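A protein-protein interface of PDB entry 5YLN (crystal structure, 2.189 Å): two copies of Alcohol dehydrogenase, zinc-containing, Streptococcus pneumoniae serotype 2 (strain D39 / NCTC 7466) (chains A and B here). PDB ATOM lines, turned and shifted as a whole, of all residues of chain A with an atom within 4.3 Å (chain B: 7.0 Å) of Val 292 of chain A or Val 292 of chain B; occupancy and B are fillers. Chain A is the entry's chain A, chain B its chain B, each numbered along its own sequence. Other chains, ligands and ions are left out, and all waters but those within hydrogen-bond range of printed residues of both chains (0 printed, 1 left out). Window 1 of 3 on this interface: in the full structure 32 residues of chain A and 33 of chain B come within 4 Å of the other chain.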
ATOM      1  N   PHE A 255     -19.339 -20.642  -1.473  1.00  0.00           N
ATOM      2  CA  PHE A 255     -19.026 -19.417  -0.754  1.00  0.00           C
ATOM      3  C   PHE A 255     -20.217 -18.480  -0.771  1.00  0.00           C
ATOM      4  O   PHE A 255     -20.528 -17.837   0.240  1.00  0.00           O
ATOM      5  CB  PHE A 255     -17.807 -18.704  -1.336  1.00  0.00           C
ATOM      6  CG  PHE A 255     -17.511 -17.384  -0.648  1.00  0.00           C
ATOM      7  CD1 PHE A 255     -16.775 -17.346   0.540  1.00  0.00           C
ATOM      8  CD2 PHE A 255     -18.009 -16.186  -1.154  1.00  0.00           C
ATOM      9  CE1 PHE A 255     -16.520 -16.151   1.187  1.00  0.00           C
ATOM     10  CE2 PHE A 255     -17.752 -14.980  -0.513  1.00  0.00           C
ATOM     11  CZ  PHE A 255     -17.008 -14.968   0.661  1.00  0.00           C
ATOM     12  N   VAL A 268     -18.078 -16.969   8.586  1.00  0.00           N
ATOM     13  CA  VAL A 268     -17.906 -17.891   7.464  1.00  0.00           C
ATOM     14  C   VAL A 268     -16.463 -18.377   7.522  1.00  0.00           C
ATOM     15  O   VAL A 268     -15.530 -17.590   7.333  1.00  0.00           O
ATOM     16  CB  VAL A 268     -18.208 -17.212   6.122  1.00  0.00           C
ATOM     17  CG1 VAL A 268     -17.996 -18.193   4.943  1.00  0.00           C
ATOM     18  CG2 VAL A 268     -19.629 -16.638   6.101  1.00  0.00           C
ATOM     19  N   PHE A 280     -17.728 -11.104  -2.967  1.00  0.00           N
ATOM     20  CA  PHE A 280     -18.046 -10.856  -1.568  1.00  0.00           C
ATOM     21  C   PHE A 280     -19.033  -9.691  -1.494  1.00  0.00           C
ATOM     22  O   PHE A 280     -18.709  -8.581  -1.921  1.00  0.00           O
ATOM     23  CB  PHE A 280     -16.748 -10.564  -0.815  1.00  0.00           C
ATOM     24  CG  PHE A 280     -16.919 -10.367   0.631  1.00  0.00           C
ATOM     25  CD1 PHE A 280     -17.787 -11.172   1.354  1.00  0.00           C
ATOM     26  CD2 PHE A 280     -16.182  -9.400   1.295  1.00  0.00           C
ATOM     27  CE1 PHE A 280     -17.943 -10.991   2.707  1.00  0.00           C
ATOM     28  CE2 PHE A 280     -16.335  -9.220   2.658  1.00  0.00           C
ATOM     29  CZ  PHE A 280     -17.214 -10.015   3.359  1.00  0.00           C
ATOM     30  N   ILE A 290     -20.063  -9.475  10.352  1.00  0.00           N
ATOM     31  CA  ILE A 290     -19.655 -10.844  10.060  1.00  0.00           C
ATOM     32  C   ILE A 290     -18.144 -10.917   9.881  1.00  0.00           C
ATOM     33  O   ILE A 290     -17.448  -9.913   9.728  1.00  0.00           O
ATOM     34  CB  ILE A 290     -20.377 -11.415   8.833  1.00  0.00           C
ATOM     35  CG1 ILE A 290     -19.984 -10.612   7.593  1.00  0.00           C
ATOM     36  CG2 ILE A 290     -21.893 -11.472   9.068  1.00  0.00           C
ATOM     37  CD1 ILE A 290     -19.880 -11.447   6.368  1.00  0.00           C
ATOM     38  N   ASN A 291     -17.647 -12.132   9.910  1.00  0.00           N
ATOM     39  CA  ASN A 291     -16.245 -12.429   9.727  1.00  0.00           C
ATOM     40  C   ASN A 291     -16.132 -13.480   8.634  1.00  0.00           C
ATOM     41  O   ASN A 291     -17.033 -14.302   8.434  1.00  0.00           O
ATOM     42  CB  ASN A 291     -15.595 -12.955  11.040  1.00  0.00           C
ATOM     43  CG  ASN A 291     -15.935 -12.108  12.242  1.00  0.00           C
ATOM     44  OD1 ASN A 291     -15.499 -10.966  12.345  1.00  0.00           O
ATOM     45  ND2 ASN A 291     -16.707 -12.674  13.176  1.00  0.00           N
ATOM     46  N   VAL A 292     -15.019 -13.452   7.923  1.00  0.00           N
ATOM     47  CA  VAL A 292     -14.696 -14.490   6.961  1.00  0.00           C
ATOM     48  C   VAL A 292     -13.275 -14.906   7.267  1.00  0.00           C
ATOM     49  O   VAL A 292     -12.379 -14.056   7.308  1.00  0.00           O
ATOM     50  CB  VAL A 292     -14.827 -14.002   5.505  1.00  0.00           C
ATOM     51  CG1 VAL A 292     -14.483 -15.132   4.525  1.00  0.00           C
ATOM     52  CG2 VAL A 292     -16.244 -13.424   5.242  1.00  0.00           C
ATOM     53  N   THR A 293     -13.065 -16.187   7.532  1.00  0.00           N
ATOM     54  CA  THR A 293     -11.721 -16.655   7.820  1.00  0.00           C
ATOM     55  C   THR A 293     -11.273 -17.641   6.759  1.00  0.00           C
ATOM     56  O   THR A 293     -12.074 -18.378   6.189  1.00  0.00           O
ATOM     57  CB  THR A 293     -11.607 -17.317   9.201  1.00  0.00           C
ATOM     58  OG1 THR A 293     -12.436 -18.486   9.240  1.00  0.00           O
ATOM     59  CG2 THR A 293     -12.020 -16.333  10.338  1.00  0.00           C
ATOM     60  N   PHE B 255     -10.750  -1.887  -0.739  1.00  0.00           N
ATOM     61  CA  PHE B 255     -10.793  -3.273  -0.275  1.00  0.00           C
ATOM     62  C   PHE B 255      -9.740  -4.121  -0.978  1.00  0.00           C
ATOM     63  O   PHE B 255      -9.101  -4.981  -0.352  1.00  0.00           O
ATOM     64  CB  PHE B 255     -12.171  -3.898  -0.500  1.00  0.00           C
ATOM     65  CG  PHE B 255     -12.234  -5.364  -0.103  1.00  0.00           C
ATOM     66  CD1 PHE B 255     -12.514  -5.725   1.208  1.00  0.00           C
ATOM     67  CD2 PHE B 255     -11.989  -6.377  -1.034  1.00  0.00           C
ATOM     68  CE1 PHE B 255     -12.552  -7.064   1.595  1.00  0.00           C
ATOM     69  CE2 PHE B 255     -12.031  -7.726  -0.658  1.00  0.00           C
ATOM     70  CZ  PHE B 255     -12.320  -8.065   0.666  1.00  0.00           C
ATOM     71  N   GLN B 259      -6.578  -6.261   0.728  1.00  0.00           N
ATOM     72  CA  GLN B 259      -6.388  -7.699   0.577  1.00  0.00           C
ATOM     73  C   GLN B 259      -5.075  -8.040  -0.112  1.00  0.00           C
ATOM     74  O   GLN B 259      -4.654  -9.197  -0.065  1.00  0.00           O
ATOM     75  CB  GLN B 259      -7.564  -8.324  -0.188  1.00  0.00           C
ATOM     76  CG  GLN B 259      -7.495  -8.196  -1.702  1.00  0.00           C
ATOM     77  CD  GLN B 259      -8.623  -8.961  -2.394  1.00  0.00           C
ATOM     78  OE1 GLN B 259      -9.117  -9.973  -1.886  1.00  0.00           O
ATOM     79  NE2 GLN B 259      -9.026  -8.481  -3.558  1.00  0.00           N
ATOM     80  N   GLY B 266      -3.107 -12.077   9.394  1.00  0.00           N
ATOM     81  CA  GLY B 266      -3.599 -10.738   9.607  1.00  0.00           C
ATOM     82  C   GLY B 266      -5.089 -10.594   9.345  1.00  0.00           C
ATOM     83  O   GLY B 266      -5.766 -11.474   8.807  1.00  0.00           O
ATOM     84  N   THR B 267      -5.604  -9.434   9.725  1.00  0.00           N
ATOM     85  CA  THR B 267      -7.024  -9.146   9.603  1.00  0.00           C
ATOM     86  C   THR B 267      -7.209  -7.909   8.744  1.00  0.00           C
ATOM     87  O   THR B 267      -6.542  -6.890   8.960  1.00  0.00           O
ATOM     88  CB  THR B 267      -7.664  -8.969  10.992  1.00  0.00           C
ATOM     89  OG1 THR B 267      -7.542 -10.203  11.722  1.00  0.00           O
ATOM     90  CG2 THR B 267      -9.137  -8.587  10.875  1.00  0.00           C
ATOM     91  N   VAL B 268      -8.091  -8.020   7.755  1.00  0.00           N
ATOM     92  CA  VAL B 268      -8.599  -6.873   7.016  1.00  0.00           C
ATOM     93  C   VAL B 268      -9.866  -6.425   7.726  1.00  0.00           C
ATOM     94  O   VAL B 268     -10.881  -7.124   7.686  1.00  0.00           O
ATOM     95  CB  VAL B 268      -8.889  -7.214   5.548  1.00  0.00           C
ATOM     96  CG1 VAL B 268      -9.399  -5.972   4.822  1.00  0.00           C
ATOM     97  CG2 VAL B 268      -7.659  -7.777   4.865  1.00  0.00           C
ATOM     98  N   ALA B 269      -9.807  -5.260   8.371  1.00  0.00           N
ATOM     99  CA  ALA B 269     -10.921  -4.717   9.150  1.00  0.00           C
ATOM    100  C   ALA B 269     -11.644  -3.678   8.305  1.00  0.00           C
ATOM    101  O   ALA B 269     -11.098  -2.610   8.010  1.00  0.00           O
ATOM    102  CB  ALA B 269     -10.437  -4.094  10.459  1.00  0.00           C
ATOM    103  N   ASN B 270     -12.871  -3.977   7.925  1.00  0.00           N
ATOM    104  CA  ASN B 270     -13.644  -3.060   7.118  1.00  0.00           C
ATOM    105  C   ASN B 270     -14.594  -2.271   8.007  1.00  0.00           C
ATOM    106  O   ASN B 270     -15.465  -2.859   8.656  1.00  0.00           O
ATOM    107  CB  ASN B 270     -14.426  -3.807   6.043  1.00  0.00           C
ATOM    108  CG  ASN B 270     -15.091  -2.864   5.120  1.00  0.00           C
ATOM    109  OD1 ASN B 270     -14.435  -2.260   4.281  1.00  0.00           O
ATOM    110  ND2 ASN B 270     -16.382  -2.634   5.333  1.00  0.00           N
ATOM    111  N   PHE B 280     -13.081 -10.716  -4.012  1.00  0.00           N
ATOM    112  CA  PHE B 280     -12.326 -11.216  -2.876  1.00  0.00           C
ATOM    113  C   PHE B 280     -11.461 -12.358  -3.389  1.00  0.00           C
ATOM    114  O   PHE B 280     -11.988 -13.362  -3.882  1.00  0.00           O
ATOM    115  CB  PHE B 280     -13.298 -11.654  -1.776  1.00  0.00           C
ATOM    116  CG  PHE B 280     -12.655 -12.291  -0.583  1.00  0.00           C
ATOM    117  CD1 PHE B 280     -11.528 -11.743   0.003  1.00  0.00           C
ATOM    118  CD2 PHE B 280     -13.224 -13.417  -0.015  1.00  0.00           C
ATOM    119  CE1 PHE B 280     -10.946 -12.339   1.114  1.00  0.00           C
ATOM    120  CE2 PHE B 280     -12.655 -14.016   1.098  1.00  0.00           C
ATOM    121  CZ  PHE B 280     -11.516 -13.475   1.668  1.00  0.00           C
ATOM    122  N   LEU B 282     -10.019 -15.133  -2.879  1.00  0.00           N
ATOM    123  CA  LEU B 282      -9.900 -16.388  -2.137  1.00  0.00           C
ATOM    124  C   LEU B 282      -8.964 -17.380  -2.813  1.00  0.00           C
ATOM    125  O   LEU B 282      -8.435 -18.268  -2.133  1.00  0.00           O
ATOM    126  CB  LEU B 282     -11.275 -17.050  -1.951  1.00  0.00           C
ATOM    127  CG  LEU B 282     -12.033 -16.963  -0.634  1.00  0.00           C
ATOM    128  CD1 LEU B 282     -13.229 -17.904  -0.686  1.00  0.00           C
ATOM    129  CD2 LEU B 282     -11.127 -17.281   0.565  1.00  0.00           C
ATOM    130  N   LEU B 285      -5.888 -16.252  -1.209  1.00  0.00           N
ATOM    131  CA  LEU B 285      -5.906 -15.976   0.224  1.00  0.00           C
ATOM    132  C   LEU B 285      -6.422 -17.131   1.074  1.00  0.00           C
ATOM    133  O   LEU B 285      -6.334 -17.052   2.304  1.00  0.00           O
ATOM    134  CB  LEU B 285      -6.761 -14.728   0.492  1.00  0.00           C
ATOM    135  CG  LEU B 285      -6.226 -13.479  -0.206  1.00  0.00           C
ATOM    136  CD1 LEU B 285      -7.293 -12.393  -0.309  1.00  0.00           C
ATOM    137  CD2 LEU B 285      -4.995 -12.965   0.537  1.00  0.00           C
ATOM    138  N   ILE B 290      -5.962 -15.595   6.602  1.00  0.00           N
ATOM    139  CA  ILE B 290      -6.376 -14.225   6.862  1.00  0.00           C
ATOM    140  C   ILE B 290      -7.829 -14.201   7.313  1.00  0.00           C
ATOM    141  O   ILE B 290      -8.549 -15.197   7.239  1.00  0.00           O
ATOM    142  CB  ILE B 290      -6.121 -13.293   5.651  1.00  0.00           C
ATOM    143  CG1 ILE B 290      -6.837 -13.776   4.380  1.00  0.00           C
ATOM    144  CG2 ILE B 290      -4.610 -13.157   5.434  1.00  0.00           C
ATOM    145  CD1 ILE B 290      -8.235 -13.217   4.201  1.00  0.00           C
ATOM    146  N   ASN B 291      -8.233 -13.052   7.850  1.00  0.00           N
ATOM    147  CA  ASN B 291      -9.581 -12.797   8.321  1.00  0.00           C
ATOM    148  C   ASN B 291     -10.042 -11.476   7.730  1.00  0.00           C
ATOM    149  O   ASN B 291      -9.246 -10.537   7.605  1.00  0.00           O
ATOM    150  CB  ASN B 291      -9.639 -12.727   9.865  1.00  0.00           C
ATOM    151  CG  ASN B 291      -8.812 -13.806  10.521  1.00  0.00           C
ATOM    152  OD1 ASN B 291      -9.193 -14.968  10.525  1.00  0.00           O
ATOM    153  ND2 ASN B 291      -7.668 -13.423  11.078  1.00  0.00           N
ATOM    154  N   VAL B 292     -11.320 -11.411   7.365  1.00  0.00           N
ATOM    155  CA  VAL B 292     -11.972 -10.192   6.901  1.00  0.00           C
ATOM    156  C   VAL B 292     -13.131  -9.947   7.839  1.00  0.00           C
ATOM    157  O   VAL B 292     -13.996 -10.816   7.982  1.00  0.00           O
ATOM    158  CB  VAL B 292     -12.476 -10.313   5.451  1.00  0.00           C
ATOM    159  CG1 VAL B 292     -13.065  -8.988   4.974  1.00  0.00           C
ATOM    160  CG2 VAL B 292     -11.369 -10.800   4.528  1.00  0.00           C
ATOM    161  N   THR B 293     -13.155  -8.783   8.481  1.00  0.00           N
ATOM    162  CA  THR B 293     -14.237  -8.439   9.390  1.00  0.00           C
ATOM    163  C   THR B 293     -15.021  -7.238   8.870  1.00  0.00           C
ATOM    164  O   THR B 293     -14.480  -6.360   8.194  1.00  0.00           O
ATOM    165  CB  THR B 293     -13.715  -8.117  10.796  1.00  0.00           C
ATOM    166  OG1 THR B 293     -12.850  -6.981  10.730  1.00  0.00           O
ATOM    167  CG2 THR B 293     -12.965  -9.331  11.432  1.00  0.00           C
ATOM    168  N   THR B 294     -16.302  -7.200   9.219  1.00  0.00           N
ATOM    169  CA  THR B 294     -17.181  -6.073   8.926  1.00  0.00           C
ATOM    170  C   THR B 294     -17.917  -5.700  10.209  1.00  0.00           C
ATOM    171  O   THR B 294     -17.777  -6.359  11.246  1.00  0.00           O
ATOM    172  CB  THR B 294     -18.203  -6.396   7.821  1.00  0.00           C
ATOM    173  OG1 THR B 294     -19.267  -7.195   8.377  1.00  0.00           O
ATOM    174  CG2 THR B 294     -17.551  -7.156   6.670  1.00  0.00           C
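Of the printed residues of chain B, Asn 291 of chain A touches Val 292 and Thr 293.
Of the printed residues of chain B, Val 292 of chain A touches Ile 290 (3.997 Å), Asn 291 (3.2 Å) and Val 292 (2.8 Å).
Val 268 of chain B touches none of the printed residues of chain A.
Printed residues of chain A within 4 Å of Phe 280 of chain B: Phe 280.
Of the printed residues of chain A, Val 292 of chain B touches Ile 290 (3.97 Å), Asn 291 (3.3 Å) and Val 292 (2.8 Å).
Printed residues of chain A within 4 Å of Thr 293 of chain B: Ile 290 and Asn 291.
The nearest printed residue of chain B that does not touch Phe 255 of chain A is Phe 280 of chain B (4.1 Å).
The backbone carbonyl oxygen (O) of Val 292 of chain B lies within hydrogen-bond range of the backbone NH (N) of Val 292 of chain A.
O of Ile 290 of chain A sits at hydrogen-bond distance from N of Thr 294 of chain B (3.0 Å).
The backbone carbonyl oxygen (O) of Thr 293 of chain B lies within hydrogen-bond range of the backbone NH (N) of Asn 270 of chain B, 2.9 Å away.
N of Thr 293 of chain B is in hydrogen-bond range of O of Val 268 of chain B, at 2.9 Å.
N of Val 268 of chain A sits at hydrogen-bond distance from O of Asn 291 of chain A, 2.9 Å away.
The backbone carbonyl oxygen (O) of Val 268 of chain A is in hydrogen-bond range of the backbone NH (N) of Thr 293 of chain A (2.8 Å).
O of Gly 266 of chain B sits at hydrogen-bond distance from N of Asn 291 of chain B, at 3.1 Å.
The side-chain hydroxyl (OG1) of Thr 267 of chain B is in hydrogen-bond range of the side-chain amide nitrogen (ND2) of Asn 291 of chain B.
Among the printed residues, pairs that only touch across the chains: Phe 255 of chain A with Leu 282 of chain B (3.8 Å), Phe 280 of chain A with Phe 280 of chain B (3.7 Å), Ile 290 of chain A with Val 292 of chain B (3.97 Å), Ile 290 of chain A with Thr 293 of chain B (3.5 Å), Asn 291 of chain A with Val 292 of chain B (3.3 Å), Asn 291 of chain A with Thr 293 of chain B (3.2 Å), Val 292 of chain A with Ile 290 of chain B (3.997 Å), Val 292 of chain A with Asn 291 of chain B (3.2 Å), Thr 293 of chain A with Ile 290 of chain B (3.5 Å) and Thr 293 of chain A with Asn 291 of chain B (3.1 Å).
Phe 280 of chain A touches its own counterpart, Phe 280 of chain B.
Ile 290 of chain A touches Thr 293 of chain B, and with the chains exchanged Thr 293 of chain A touches Ile 290 of chain B.
Asn 291 of chain A touches Val 292 of chain B, and with the chains exchanged Val 292 of chain A touches Asn 291 of chain B.
Asn 291 of chain A touches Thr 293 of chain B, and with the chains exchanged Thr 293 of chain A touches Asn 291 of chain B.
7 positions are printed for both chains.
Of the 12 pairs that touch across the chains among the printed residues, 10 have their exchanged pair printed and touching as well.
Of the 7 printed residues of chain A, 6 touch a printed residue of chain B.
Hydrophobic or aromatic side chains of chain A within 4 Å of the printed part of chain B: Phe 255, Phe 280 and Ile 290.
Along chain A the printed residues that touch a printed residue of chain B span positions 255 to 293.
Hydrophobic or aromatic side chains of chain B that line the printed part of chain A: Phe 280 and Leu 282.
Among the printed residues, no Asp or Glu carboxylate lies within 4 Å of a Lys or Arg side-chain nitrogen of the other chain.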
